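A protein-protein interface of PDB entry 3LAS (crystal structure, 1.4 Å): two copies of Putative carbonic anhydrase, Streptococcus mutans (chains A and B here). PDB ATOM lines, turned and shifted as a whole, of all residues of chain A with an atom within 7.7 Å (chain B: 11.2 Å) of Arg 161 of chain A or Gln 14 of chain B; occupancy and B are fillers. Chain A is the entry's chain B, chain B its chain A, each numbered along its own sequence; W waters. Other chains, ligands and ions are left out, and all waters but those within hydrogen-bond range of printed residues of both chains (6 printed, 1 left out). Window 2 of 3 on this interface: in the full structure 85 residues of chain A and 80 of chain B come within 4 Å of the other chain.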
ATOM      1  N   PRO A  47      18.349  23.536   4.797  1.00  0.00           N
ATOM      2  CA  PRO A  47      17.099  22.785   5.027  1.00  0.00           C
ATOM      3  C   PRO A  47      16.732  21.868   3.871  1.00  0.00           C
ATOM      4  O   PRO A  47      16.169  20.820   4.088  1.00  0.00           O
ATOM      5  CB  PRO A  47      16.009  23.887   5.276  1.00  0.00           C
ATOM      6  CG  PRO A  47      16.636  25.112   4.712  1.00  0.00           C
ATOM      7  CD  PRO A  47      18.120  24.992   4.926  1.00  0.00           C
ATOM      8  N   ALA A  48      17.061  22.306   2.650  1.00  0.00           N
ATOM      9  CA  ALA A  48      16.718  21.447   1.506  1.00  0.00           C
ATOM     10  C   ALA A  48      17.366  20.111   1.560  1.00  0.00           C
ATOM     11  O   ALA A  48      16.806  19.117   1.093  1.00  0.00           O
ATOM     12  CB  ALA A  48      17.057  22.159   0.229  1.00  0.00           C
ATOM     13  N   LEU A  49      18.588  20.051   2.104  1.00  0.00           N
ATOM     14  CA  LEU A  49      19.364  18.780   2.139  1.00  0.00           C
ATOM     15  C   LEU A  49      19.510  18.232   3.571  1.00  0.00           C
ATOM     16  O   LEU A  49      20.179  17.170   3.704  1.00  0.00           O
ATOM     17  CB  LEU A  49      20.766  18.966   1.498  1.00  0.00           C
ATOM     18  CG  LEU A  49      20.759  19.523   0.108  1.00  0.00           C
ATOM     19  CD1 LEU A  49      22.166  19.648  -0.406  1.00  0.00           C
ATOM     20  CD2 LEU A  49      19.942  18.683  -0.876  1.00  0.00           C
ATOM     21  N   LEU A  89      24.397  20.782  -8.189  1.00  0.00           N
ATOM     22  CA  LEU A  89      22.924  20.970  -7.987  1.00  0.00           C
ATOM     23  C   LEU A  89      22.520  22.155  -8.781  1.00  0.00           C
ATOM     24  O   LEU A  89      22.857  23.314  -8.475  1.00  0.00           O
ATOM     25  CB  LEU A  89      22.676  21.130  -6.445  1.00  0.00           C
ATOM     26  CG  LEU A  89      21.230  21.459  -6.135  1.00  0.00           C
ATOM     27  CD1 LEU A  89      20.314  20.234  -6.462  1.00  0.00           C
ATOM     28  CD2 LEU A  89      21.137  21.798  -4.646  1.00  0.00           C
ATOM     29  N   HIS A  90      21.810  21.946  -9.898  1.00  0.00           N
ATOM     30  CA  HIS A  90      21.162  23.061 -10.624  1.00  0.00           C
ATOM     31  C   HIS A  90      19.709  23.170 -10.206  1.00  0.00           C
ATOM     32  O   HIS A  90      19.307  22.430  -9.293  1.00  0.00           O
ATOM     33  CB  HIS A  90      21.341  22.931 -12.112  1.00  0.00           C
ATOM     34  CG  HIS A  90      22.769  23.071 -12.560  1.00  0.00           C
ATOM     35  ND1 HIS A  90      23.917  23.317 -11.777  1.00  0.00           N
ATOM     36  CD2 HIS A  90      23.186  22.999 -13.850  1.00  0.00           C
ATOM     37  CE1 HIS A  90      25.003  23.357 -12.598  1.00  0.00           C
ATOM     38  NE2 HIS A  90      24.555  23.195 -13.839  1.00  0.00           N
ATOM     39  N   HIS A  91      18.908  24.065 -10.795  1.00  0.00           N
ATOM     40  CA  HIS A  91      17.540  24.188 -10.325  1.00  0.00           C
ATOM     41  C   HIS A  91      16.641  24.711 -11.402  1.00  0.00           C
ATOM     42  O   HIS A  91      17.136  25.270 -12.442  1.00  0.00           O
ATOM     43  CB  HIS A  91      17.494  25.095  -9.085  1.00  0.00           C
ATOM     44  CG  HIS A  91      17.778  26.538  -9.386  1.00  0.00           C
ATOM     45  ND1 HIS A  91      16.765  27.416  -9.681  1.00  0.00           N
ATOM     46  CD2 HIS A  91      18.933  27.235  -9.550  1.00  0.00           C
ATOM     47  CE1 HIS A  91      17.253  28.614 -10.002  1.00  0.00           C
ATOM     48  NE2 HIS A  91      18.574  28.523  -9.962  1.00  0.00           N
ATOM     49  N   THR A  92      15.337  24.581 -11.204  1.00  0.00           N
ATOM     50  CA  THR A  92      14.329  25.040 -12.162  1.00  0.00           C
ATOM     51  C   THR A  92      14.173  26.556 -12.022  1.00  0.00           C
ATOM     52  O   THR A  92      14.371  27.179 -10.985  1.00  0.00           O
ATOM     53  CB  THR A  92      12.986  24.335 -11.925  1.00  0.00           C
ATOM     54  OG1 THR A  92      12.531  24.644 -10.628  1.00  0.00           O
ATOM     55  CG2 THR A  92      13.104  22.831 -12.150  1.00  0.00           C
ATOM     56  N   ALA A 153      22.243  16.748  -9.603  1.00  0.00           N
ATOM     57  CA  ALA A 153      20.845  16.842  -9.132  1.00  0.00           C
ATOM     58  C   ALA A 153      20.236  18.142  -9.571  1.00  0.00           C
ATOM     59  O   ALA A 153      20.975  19.104  -9.944  1.00  0.00           O
ATOM     60  CB  ALA A 153      20.789  16.750  -7.599  1.00  0.00           C
ATOM     61  N   ILE A 154      18.914  18.214  -9.492  1.00  0.00           N
ATOM     62  CA  ILE A 154      18.105  19.419  -9.795  1.00  0.00           C
ATOM     63  C   ILE A 154      17.167  19.689  -8.665  1.00  0.00           C
ATOM     64  O   ILE A 154      16.489  18.789  -8.175  1.00  0.00           O
ATOM     65  CB  ILE A 154      17.353  19.244 -11.106  1.00  0.00           C
ATOM     66  CG1 ILE A 154      18.377  19.166 -12.262  1.00  0.00           C
ATOM     67  CG2 ILE A 154      16.371  20.470 -11.325  1.00  0.00           C
ATOM     68  CD1 ILE A 154      17.755  18.754 -13.625  1.00  0.00           C
ATOM     69  N   TYR A 155      17.116  20.909  -8.180  1.00  0.00           N
ATOM     70  CA  TYR A 155      16.156  21.414  -7.199  1.00  0.00           C
ATOM     71  C   TYR A 155      15.009  22.124  -7.849  1.00  0.00           C
ATOM     72  O   TYR A 155      15.241  22.988  -8.730  1.00  0.00           O
ATOM     73  CB  TYR A 155      16.905  22.427  -6.327  1.00  0.00           C
ATOM     74  CG  TYR A 155      16.056  23.094  -5.287  1.00  0.00           C
ATOM     75  CD1 TYR A 155      15.630  22.372  -4.132  1.00  0.00           C
ATOM     76  CD2 TYR A 155      15.683  24.414  -5.408  1.00  0.00           C
ATOM     77  CE1 TYR A 155      14.836  22.965  -3.151  1.00  0.00           C
ATOM     78  CE2 TYR A 155      14.903  25.064  -4.388  1.00  0.00           C
ATOM     79  CZ  TYR A 155      14.518  24.299  -3.313  1.00  0.00           C
ATOM     80  OH  TYR A 155      13.697  24.875  -2.356  1.00  0.00           O
ATOM     81  N   ASP A 156      13.780  21.754  -7.501  1.00  0.00           N
ATOM     82  CA  ASP A 156      12.602  22.399  -8.065  1.00  0.00           C
ATOM     83  C   ASP A 156      12.236  23.526  -7.122  1.00  0.00           C
ATOM     84  O   ASP A 156      11.846  23.290  -5.968  1.00  0.00           O
ATOM     85  CB  ASP A 156      11.505  21.332  -8.210  1.00  0.00           C
ATOM     86  CG  ASP A 156      10.252  21.876  -8.789  1.00  0.00           C
ATOM     87  OD1 ASP A 156       9.836  23.016  -8.490  1.00  0.00           O
ATOM     88  OD2 ASP A 156       9.575  21.147  -9.581  1.00  0.00           O
ATOM     89  N   VAL A 157      12.364  24.765  -7.556  1.00  0.00           N
ATOM     90  CA  VAL A 157      12.164  25.917  -6.652  1.00  0.00           C
ATOM     91  C   VAL A 157      10.724  26.054  -6.186  1.00  0.00           C
ATOM     92  O   VAL A 157      10.462  26.685  -5.165  1.00  0.00           O
ATOM     93  CB  VAL A 157      12.594  27.254  -7.253  1.00  0.00           C
ATOM     94  CG1 VAL A 157      14.108  27.296  -7.424  1.00  0.00           C
ATOM     95  CG2 VAL A 157      11.866  27.568  -8.579  1.00  0.00           C
ATOM     96  N   ASP A 158       9.762  25.439  -6.893  1.00  0.00           N
ATOM     97  CA  ASP A 158       8.331  25.558  -6.460  1.00  0.00           C
ATOM     98  C   ASP A 158       7.946  24.484  -5.533  1.00  0.00           C
ATOM     99  O   ASP A 158       6.955  24.719  -4.753  1.00  0.00           O
ATOM    100  CB  ASP A 158       7.448  25.496  -7.716  1.00  0.00           C
ATOM    101  CG  ASP A 158       7.684  26.707  -8.563  1.00  0.00           C
ATOM    102  OD1 ASP A 158       8.174  27.809  -8.141  1.00  0.00           O
ATOM    103  OD2 ASP A 158       7.521  26.482  -9.815  1.00  0.00           O
ATOM    104  N   THR A 159       8.615  23.358  -5.506  1.00  0.00           N
ATOM    105  CA  THR A 159       8.201  22.254  -4.599  1.00  0.00           C
ATOM    106  C   THR A 159       9.182  21.935  -3.496  1.00  0.00           C
ATOM    107  O   THR A 159       8.791  21.249  -2.520  1.00  0.00           O
ATOM    108  CB  THR A 159       7.922  20.942  -5.371  1.00  0.00           C
ATOM    109  OG1 THR A 159       9.212  20.502  -5.926  1.00  0.00           O
ATOM    110  CG2 THR A 159       6.944  21.143  -6.526  1.00  0.00           C
ATOM    111  N   GLY A 160      10.431  22.385  -3.619  1.00  0.00           N
ATOM    112  CA  GLY A 160      11.464  22.007  -2.665  1.00  0.00           C
ATOM    113  C   GLY A 160      12.163  20.719  -2.975  1.00  0.00           C
ATOM    114  O   GLY A 160      13.076  20.371  -2.247  1.00  0.00           O
ATOM    115  N   ARG A 161      11.743  19.997  -4.043  1.00  0.00           N
ATOM    116  CA  ARG A 161      12.283  18.676  -4.298  1.00  0.00           C
ATOM    117  C   ARG A 161      13.654  18.660  -4.963  1.00  0.00           C
ATOM    118  O   ARG A 161      13.846  19.402  -5.963  1.00  0.00           O
ATOM    119  CB  ARG A 161      11.287  17.950  -5.191  1.00  0.00           C
ATOM    120  CG  ARG A 161      11.742  16.518  -5.626  1.00  0.00           C
ATOM    121  CD  ARG A 161      11.781  15.468  -4.529  1.00  0.00           C
ATOM    122  NE  ARG A 161      10.412  15.103  -4.125  1.00  0.00           N
ATOM    123  CZ  ARG A 161      10.191  14.195  -3.126  1.00  0.00           C
ATOM    124  NH1 ARG A 161      11.232  13.689  -2.484  1.00  0.00           N
ATOM    125  NH2 ARG A 161       8.986  13.921  -2.817  1.00  0.00           N
ATOM    126  N   VAL A 162      14.562  17.804  -4.513  1.00  0.00           N
ATOM    127  CA  VAL A 162      15.816  17.517  -5.192  1.00  0.00           C
ATOM    128  C   VAL A 162      15.729  16.170  -5.812  1.00  0.00           C
ATOM    129  O   VAL A 162      15.332  15.216  -5.153  1.00  0.00           O
ATOM    130  CB  VAL A 162      17.016  17.573  -4.189  1.00  0.00           C
ATOM    131  CG1 VAL A 162      18.336  17.170  -4.932  1.00  0.00           C
ATOM    132  CG2 VAL A 162      17.095  18.995  -3.556  1.00  0.00           C
ATOM    133  N   ARG A 163      16.076  16.061  -7.116  1.00  0.00           N
ATOM    134  CA  ARG A 163      16.114  14.768  -7.826  1.00  0.00           C
ATOM    135  C   ARG A 163      17.425  14.583  -8.476  1.00  0.00           C
ATOM    136  O   ARG A 163      18.065  15.538  -8.916  1.00  0.00           O
ATOM    137  CB  ARG A 163      14.930  14.728  -8.860  1.00  0.00           C
ATOM    138  CG  ARG A 163      15.188  15.586 -10.074  1.00  0.00           C
ATOM    139  CD  ARG A 163      13.904  15.512 -10.998  1.00  0.00           C
ATOM    140  NE  ARG A 163      14.081  16.307 -12.203  1.00  0.00           N
ATOM    141  CZ  ARG A 163      14.678  15.932 -13.326  1.00  0.00           C
ATOM    142  NH1 ARG A 163      15.215  14.775 -13.389  1.00  0.00           N
ATOM    143  NH2 ARG A 163      14.750  16.810 -14.345  1.00  0.00           N
ATOM    144  N   GLU A 164      17.870  13.337  -8.534  1.00  0.00           N
ATOM    145  CA  GLU A 164      19.177  13.000  -9.105  1.00  0.00           C
ATOM    146  C   GLU A 164      19.177  13.068 -10.622  1.00  0.00           C
ATOM    147  O   GLU A 164      18.202  12.634 -11.275  1.00  0.00           O
ATOM    148  CB  GLU A 164      19.619  11.606  -8.623  1.00  0.00           C
ATOM    149  CG  GLU A 164      20.988  11.238  -9.150  1.00  0.00           C
ATOM    150  CD  GLU A 164      21.578   9.972  -8.580  1.00  0.00           C
ATOM    151  OE1 GLU A 164      20.953   9.269  -7.783  1.00  0.00           O
ATOM    152  OE2 GLU A 164      22.757   9.771  -8.995  1.00  0.00           O
ATOM    153  N   PHE B   6      25.354  12.007  -0.739  1.00  0.00           N
ATOM    154  CA  PHE B   6      24.288  12.443  -1.600  1.00  0.00           C
ATOM    155  C   PHE B   6      23.011  11.677  -1.314  1.00  0.00           C
ATOM    156  O   PHE B   6      21.920  12.254  -1.336  1.00  0.00           O
ATOM    157  CB  PHE B   6      24.761  12.228  -3.042  1.00  0.00           C
ATOM    158  CG  PHE B   6      23.719  12.571  -4.067  1.00  0.00           C
ATOM    159  CD1 PHE B   6      23.386  13.873  -4.288  1.00  0.00           C
ATOM    160  CD2 PHE B   6      23.026  11.568  -4.716  1.00  0.00           C
ATOM    161  CE1 PHE B   6      22.379  14.205  -5.259  1.00  0.00           C
ATOM    162  CE2 PHE B   6      22.008  11.879  -5.662  1.00  0.00           C
ATOM    163  CZ  PHE B   6      21.699  13.174  -5.939  1.00  0.00           C
ATOM    164  N   ASP B   7      23.078  10.334  -1.116  1.00  0.00           N
ATOM    165  CA  ASP B   7      21.840   9.572  -0.825  1.00  0.00           C
ATOM    166  C   ASP B   7      21.249   9.939   0.448  1.00  0.00           C
ATOM    167  O   ASP B   7      20.037  10.034   0.544  1.00  0.00           O
ATOM    168  CB  ASP B   7      22.202   8.030  -0.812  1.00  0.00           C
ATOM    169  CG  ASP B   7      22.776   7.639  -2.094  1.00  0.00           C
ATOM    170  OD1 ASP B   7      22.033   7.515  -3.153  1.00  0.00           O
ATOM    171  OD2 ASP B   7      23.988   7.489  -2.268  1.00  0.00           O
ATOM    172  N   ASN B   8      22.017  10.309   1.468  1.00  0.00           N
ATOM    173  CA  ASN B   8      21.482  10.828   2.693  1.00  0.00           C
ATOM    174  C   ASN B   8      20.722  12.117   2.410  1.00  0.00           C
ATOM    175  O   ASN B   8      19.632  12.357   2.972  1.00  0.00           O
ATOM    176  CB  ASN B   8      22.490  11.072   3.803  1.00  0.00           C
ATOM    177  CG  ASN B   8      23.261   9.927   4.259  1.00  0.00           C
ATOM    178  OD1 ASN B   8      23.997   9.330   3.487  1.00  0.00           O
ATOM    179  ND2 ASN B   8      23.335   9.786   5.617  1.00  0.00           N
ATOM    180  N   PHE B   9      21.282  13.015   1.582  1.00  0.00           N
ATOM    181  CA  PHE B   9      20.635  14.303   1.328  1.00  0.00           C
ATOM    182  C   PHE B   9      19.309  14.119   0.600  1.00  0.00           C
ATOM    183  O   PHE B   9      18.328  14.803   0.906  1.00  0.00           O
ATOM    184  CB  PHE B   9      21.571  15.175   0.443  1.00  0.00           C
ATOM    185  CG  PHE B   9      22.883  15.562   1.058  1.00  0.00           C
ATOM    186  CD1 PHE B   9      23.132  15.371   2.411  1.00  0.00           C
ATOM    187  CD2 PHE B   9      23.870  16.062   0.209  1.00  0.00           C
ATOM    188  CE1 PHE B   9      24.423  15.703   2.944  1.00  0.00           C
ATOM    189  CE2 PHE B   9      25.100  16.393   0.768  1.00  0.00           C
ATOM    190  CZ  PHE B   9      25.388  16.217   2.042  1.00  0.00           C
ATOM    191  N   ILE B  10      19.302  13.160  -0.360  1.00  0.00           N
ATOM    192  CA  ILE B  10      18.026  12.881  -1.059  1.00  0.00           C
ATOM    193  C   ILE B  10      16.960  12.414  -0.096  1.00  0.00           C
ATOM    194  O   ILE B  10      15.784  12.823  -0.151  1.00  0.00           O
ATOM    195  CB  ILE B  10      18.284  11.824  -2.170  1.00  0.00           C
ATOM    196  CG1 ILE B  10      19.059  12.445  -3.301  1.00  0.00           C
ATOM    197  CG2 ILE B  10      16.918  11.277  -2.732  1.00  0.00           C
ATOM    198  CD1 ILE B  10      18.348  13.624  -4.103  1.00  0.00           C
ATOM    199  N   LYS B  11      17.331  11.549   0.841  1.00  0.00           N
ATOM    200  CA  LYS B  11      16.332  11.085   1.830  1.00  0.00           C
ATOM    201  C   LYS B  11      15.874  12.191   2.712  1.00  0.00           C
ATOM    202  O   LYS B  11      14.674  12.323   2.929  1.00  0.00           O
ATOM    203  CB  LYS B  11      16.951   9.947   2.632  1.00  0.00           C
ATOM    204  CG  LYS B  11      16.042   9.459   3.839  1.00  0.00           C
ATOM    205  N   ALA B  12      16.771  13.031   3.200  1.00  0.00           N
ATOM    206  CA  ALA B  12      16.416  14.100   4.076  1.00  0.00           C
ATOM    207  C   ALA B  12      15.551  15.123   3.363  1.00  0.00           C
ATOM    208  O   ALA B  12      14.751  15.845   3.988  1.00  0.00           O
ATOM    209  CB  ALA B  12      17.660  14.845   4.666  1.00  0.00           C
ATOM    210  N   ASN B  13      15.736  15.257   2.067  1.00  0.00           N
ATOM    211  CA  ASN B  13      14.947  16.233   1.315  1.00  0.00           C
ATOM    212  C   ASN B  13      13.460  15.943   1.339  1.00  0.00           C
ATOM    213  O   ASN B  13      12.684  16.884   1.186  1.00  0.00           O
ATOM    214  CB  ASN B  13      15.535  16.282  -0.122  1.00  0.00           C
ATOM    215  CG  ASN B  13      14.716  17.195  -1.019  1.00  0.00           C
ATOM    216  OD1 ASN B  13      14.789  18.466  -0.868  1.00  0.00           O
ATOM    217  ND2 ASN B  13      14.031  16.656  -1.955  1.00  0.00           N
ATOM    218  N   GLN B  14      13.062  14.670   1.521  1.00  0.00           N
ATOM    219  CA  GLN B  14      11.618  14.437   1.585  1.00  0.00           C
ATOM    220  C   GLN B  14      10.888  15.272   2.663  1.00  0.00           C
ATOM    221  O   GLN B  14       9.822  15.834   2.403  1.00  0.00           O
ATOM    222  CB  GLN B  14      11.369  12.942   1.845  1.00  0.00           C
ATOM    223  CG  GLN B  14       9.835  12.626   1.970  1.00  0.00           C
ATOM    224  CD  GLN B  14       9.145  12.852   0.607  1.00  0.00           C
ATOM    225  OE1 GLN B  14       9.529  12.255  -0.409  1.00  0.00           O
ATOM    226  NE2 GLN B  14       8.041  13.685   0.579  1.00  0.00           N
ATOM    227  N   ALA B  15      11.529  15.388   3.815  1.00  0.00           N
ATOM    228  CA  ALA B  15      10.910  16.222   4.854  1.00  0.00           C
ATOM    229  C   ALA B  15      10.759  17.674   4.496  1.00  0.00           C
ATOM    230  O   ALA B  15       9.766  18.368   4.810  1.00  0.00           O
ATOM    231  CB  ALA B  15      11.668  16.099   6.147  1.00  0.00           C
ATOM    232  N   TYR B  16      11.747  18.175   3.753  1.00  0.00           N
ATOM    233  CA  TYR B  16      11.705  19.550   3.317  1.00  0.00           C
ATOM    234  C   TYR B  16      10.605  19.773   2.270  1.00  0.00           C
ATOM    235  O   TYR B  16       9.876  20.759   2.287  1.00  0.00           O
ATOM    236  CB  TYR B  16      13.053  20.012   2.724  1.00  0.00           C
ATOM    237  CG  TYR B  16      13.046  21.446   2.360  1.00  0.00           C
ATOM    238  CD1 TYR B  16      13.022  22.427   3.400  1.00  0.00           C
ATOM    239  CD2 TYR B  16      13.035  21.941   1.031  1.00  0.00           C
ATOM    240  CE1 TYR B  16      13.037  23.740   3.162  1.00  0.00           C
ATOM    241  CE2 TYR B  16      13.054  23.281   0.741  1.00  0.00           C
ATOM    242  CZ  TYR B  16      13.036  24.204   1.822  1.00  0.00           C
ATOM    243  OH  TYR B  16      13.043  25.534   1.485  1.00  0.00           O
ATOM    244  N   VAL B  17      10.471  18.801   1.340  1.00  0.00           N
ATOM    245  CA  VAL B  17       9.392  18.878   0.338  1.00  0.00           C
ATOM    246  C   VAL B  17       8.040  18.974   1.033  1.00  0.00           C
ATOM    247  O   VAL B  17       7.168  19.746   0.675  1.00  0.00           O
ATOM    248  CB  VAL B  17       9.437  17.621  -0.522  1.00  0.00           C
ATOM    249  CG1 VAL B  17       8.205  17.506  -1.431  1.00  0.00           C
ATOM    250  CG2 VAL B  17      10.669  17.728  -1.440  1.00  0.00           C
ATOM    251  N   ASP B  18       7.869  18.147   2.084  1.00  0.00           N
ATOM    252  CA  ASP B  18       6.560  18.145   2.750  1.00  0.00           C
ATOM    253  C   ASP B  18       6.293  19.480   3.437  1.00  0.00           C
ATOM    254  O   ASP B  18       5.180  19.990   3.381  1.00  0.00           O
ATOM    255  CB  ASP B  18       6.590  16.985   3.776  1.00  0.00           C
ATOM    256  CG  ASP B  18       6.543  15.592   3.112  1.00  0.00           C
ATOM    257  OD1 ASP B  18       6.190  15.407   1.948  1.00  0.00           O
ATOM    258  OD2 ASP B  18       6.898  14.685   3.865  1.00  0.00           O
ATOM    259  N   LEU B  19       7.315  20.095   4.043  1.00  0.00           N
ATOM    260  CA  LEU B  19       7.161  21.426   4.656  1.00  0.00           C
ATOM    261  C   LEU B  19       6.984  22.515   3.649  1.00  0.00           C
ATOM    262  O   LEU B  19       6.257  23.496   3.871  1.00  0.00           O
ATOM    263  CB  LEU B  19       8.423  21.711   5.512  1.00  0.00           C
ATOM    264  CG  LEU B  19       8.443  20.918   6.820  1.00  0.00           C
ATOM    265  CD1 LEU B  19       9.842  20.900   7.377  1.00  0.00           C
ATOM    266  CD2 LEU B  19       7.436  21.594   7.861  1.00  0.00           C
ATOM    267  N   HIS B  20       7.745  22.454   2.510  1.00  0.00           N
ATOM    268  CA  HIS B  20       7.762  23.574   1.573  1.00  0.00           C
ATOM    269  C   HIS B  20       6.408  23.668   0.876  1.00  0.00           C
ATOM    270  O   HIS B  20       5.944  24.757   0.518  1.00  0.00           O
ATOM    271  CB  HIS B  20       8.914  23.281   0.557  1.00  0.00           C
ATOM    272  CG  HIS B  20       9.134  24.373  -0.437  1.00  0.00           C
ATOM    273  ND1 HIS B  20       8.290  24.601  -1.526  1.00  0.00           N
ATOM    274  CD2 HIS B  20      10.131  25.309  -0.518  1.00  0.00           C
ATOM    275  CE1 HIS B  20       8.763  25.627  -2.251  1.00  0.00           C
ATOM    276  NE2 HIS B  20       9.862  26.087  -1.620  1.00  0.00           N
ATOM    277  N   GLY B  21       5.783  22.493   0.605  1.00  0.00           N
ATOM    278  CA  GLY B  21       4.585  22.451  -0.283  1.00  0.00           C
ATOM    279  C   GLY B  21       4.873  23.079  -1.642  1.00  0.00           C
ATOM    280  O   GLY B  21       6.042  23.115  -2.091  1.00  0.00           O
ATOM    281  N   THR B  22       3.852  23.484  -2.364  1.00  0.00           N
ATOM    282  CA  THR B  22       3.999  24.024  -3.711  1.00  0.00           C
ATOM    283  C   THR B  22       3.755  25.496  -3.629  1.00  0.00           C
ATOM    284  O   THR B  22       2.670  25.950  -3.242  1.00  0.00           O
ATOM    285  CB  THR B  22       2.994  23.394  -4.649  1.00  0.00           C
ATOM    286  OG1 THR B  22       3.292  22.012  -4.760  1.00  0.00           O
ATOM    287  CG2 THR B  22       3.141  24.055  -6.050  1.00  0.00           C
ATOM    288  N   ALA B  23       4.780  26.301  -3.895  1.00  0.00           N
ATOM    289  CA  ALA B  23       4.690  27.741  -3.699  1.00  0.00           C
ATOM    290  C   ALA B  23       5.787  28.358  -4.573  1.00  0.00           C
ATOM    291  O   ALA B  23       6.953  27.862  -4.521  1.00  0.00           O
ATOM    292  CB  ALA B  23       4.965  28.051  -2.234  1.00  0.00           C
ATOM    293  N   LEU B  53      13.192  32.693   2.759  1.00  0.00           N
ATOM    294  CA  LEU B  53      13.338  32.184   1.464  1.00  0.00           C
ATOM    295  C   LEU B  53      12.994  33.227   0.402  1.00  0.00           C
ATOM    296  O   LEU B  53      11.979  33.926   0.523  1.00  0.00           O
ATOM    297  CB  LEU B  53      12.464  30.901   1.324  1.00  0.00           C
ATOM    298  CG  LEU B  53      12.843  29.959   0.182  1.00  0.00           C
ATOM    299  CD1 LEU B  53      14.240  29.331   0.462  1.00  0.00           C
ATOM    300  CD2 LEU B  53      11.789  28.844   0.015  1.00  0.00           C
HETATM  301  O   HOH W   1      12.216  27.006  -3.090  1.00  0.00           O
HETATM  302  O   HOH W   2      15.311  25.878  -0.203  1.00  0.00           O
HETATM  303  O   HOH W   3       9.163  28.735  -2.944  1.00  0.00           O
HETATM  304  O   HOH W   4      14.122  13.965  -2.475  1.00  0.00           O
HETATM  305  O   HOH W   5      13.279  11.671  -0.809  1.00  0.00           O
HETATM  306  O   HOH W   6       6.195  13.522  -1.698  1.00  0.00           O
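The side-chain amide nitrogen (NE2) of Gln 14 of chain B sits at hydrogen-bond distance from the side-chain carboxylate (OD1) of Asp 18 of chain B (2.9 Å).
OG1 of Thr 159 of chain A is in hydrogen-bond range of N of Arg 161 of chain A, 3.2 Å away.
The backbone carbonyl oxygen (O) of Ala 48 of chain A lies close to the side-chain amide oxygen (OD1) of Asn 13 of chain B.
OD1 of Asn 13 of chain B sits close to O of Gly 160 of chain A, at 2.9 Å.
ND2 of Asn 13 of chain B lies close to N of Val 162 of chain A.
The side-chain amide oxygen (OE1) of Gln 14 of chain B lies within hydrogen-bond range of the guanidinium group (NH2) of Arg 161 of chain A (3.0 Å).
The backbone carbonyl oxygen of Asp 158 of chain A sits close to a ring nitrogen (ND1) of His 20 of chain B (3.5 Å).
The backbone carbonyl oxygen (O) of Asp 158 of chain A is in hydrogen-bond range of the backbone NH (N) of Ala 23 of chain B, at 2.8 Å.
O of Asp 158 of chain A lies close to O of Gly 21 of chain B, 3.2 Å away.
The backbone carbonyl oxygen of Thr 159 of chain A sits close to the backbone carbonyl oxygen of Gly 21 of chain B.
No position is printed for both chains.
Of the 26 pairs that touch across the chains among the printed residues, none has its exchanged pair printed and touching as well.
Water W6 bridges the side-chain amide nitrogen (NE2) of Gln 14 of chain B (2.9 Å) and the guanidinium group (NH2) of Arg 161 of chain A (3.0 Å).
Of the printed residues of chain B, Ala 48 of chain A touches Asn 13 (2.9 Å) and Tyr 16 (3.7 Å).
Printed residues of chain B within 4 Å of Asp 158 of chain A: His 20, Gly 21, Thr 22 and Ala 23.
Thr 159 of chain A touches three residues of chain B.
Val 162 of chain A touches just these residues of chain B: Ile 10 and Asn 13.
Gln 14 of chain B touches just one residue of chain A: Arg 161.
The nearest residue of chain B that does not touch Arg 161 of chain A is Ile 10 of chain B (5.2 Å).
The nearest residue of chain A that does not touch Gln 14 of chain B is Ala 48 of chain A (5.8 Å).
The nearest printed residue of chain A that does not touch His 20 of chain B is Tyr 155 of chain A (4.04 Å).
Hydrophobic or aromatic side chains of chain A within 4 Å of the printed part of chain B: Pro 47, Ala 153, Tyr 155 and Val 162.
Among the printed residues, 26 pairs touch across the chains.
Among the printed residues, no Asp or Glu carboxylate lies within 4 Å of a Lys or Arg side-chain nitrogen of the other chain.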
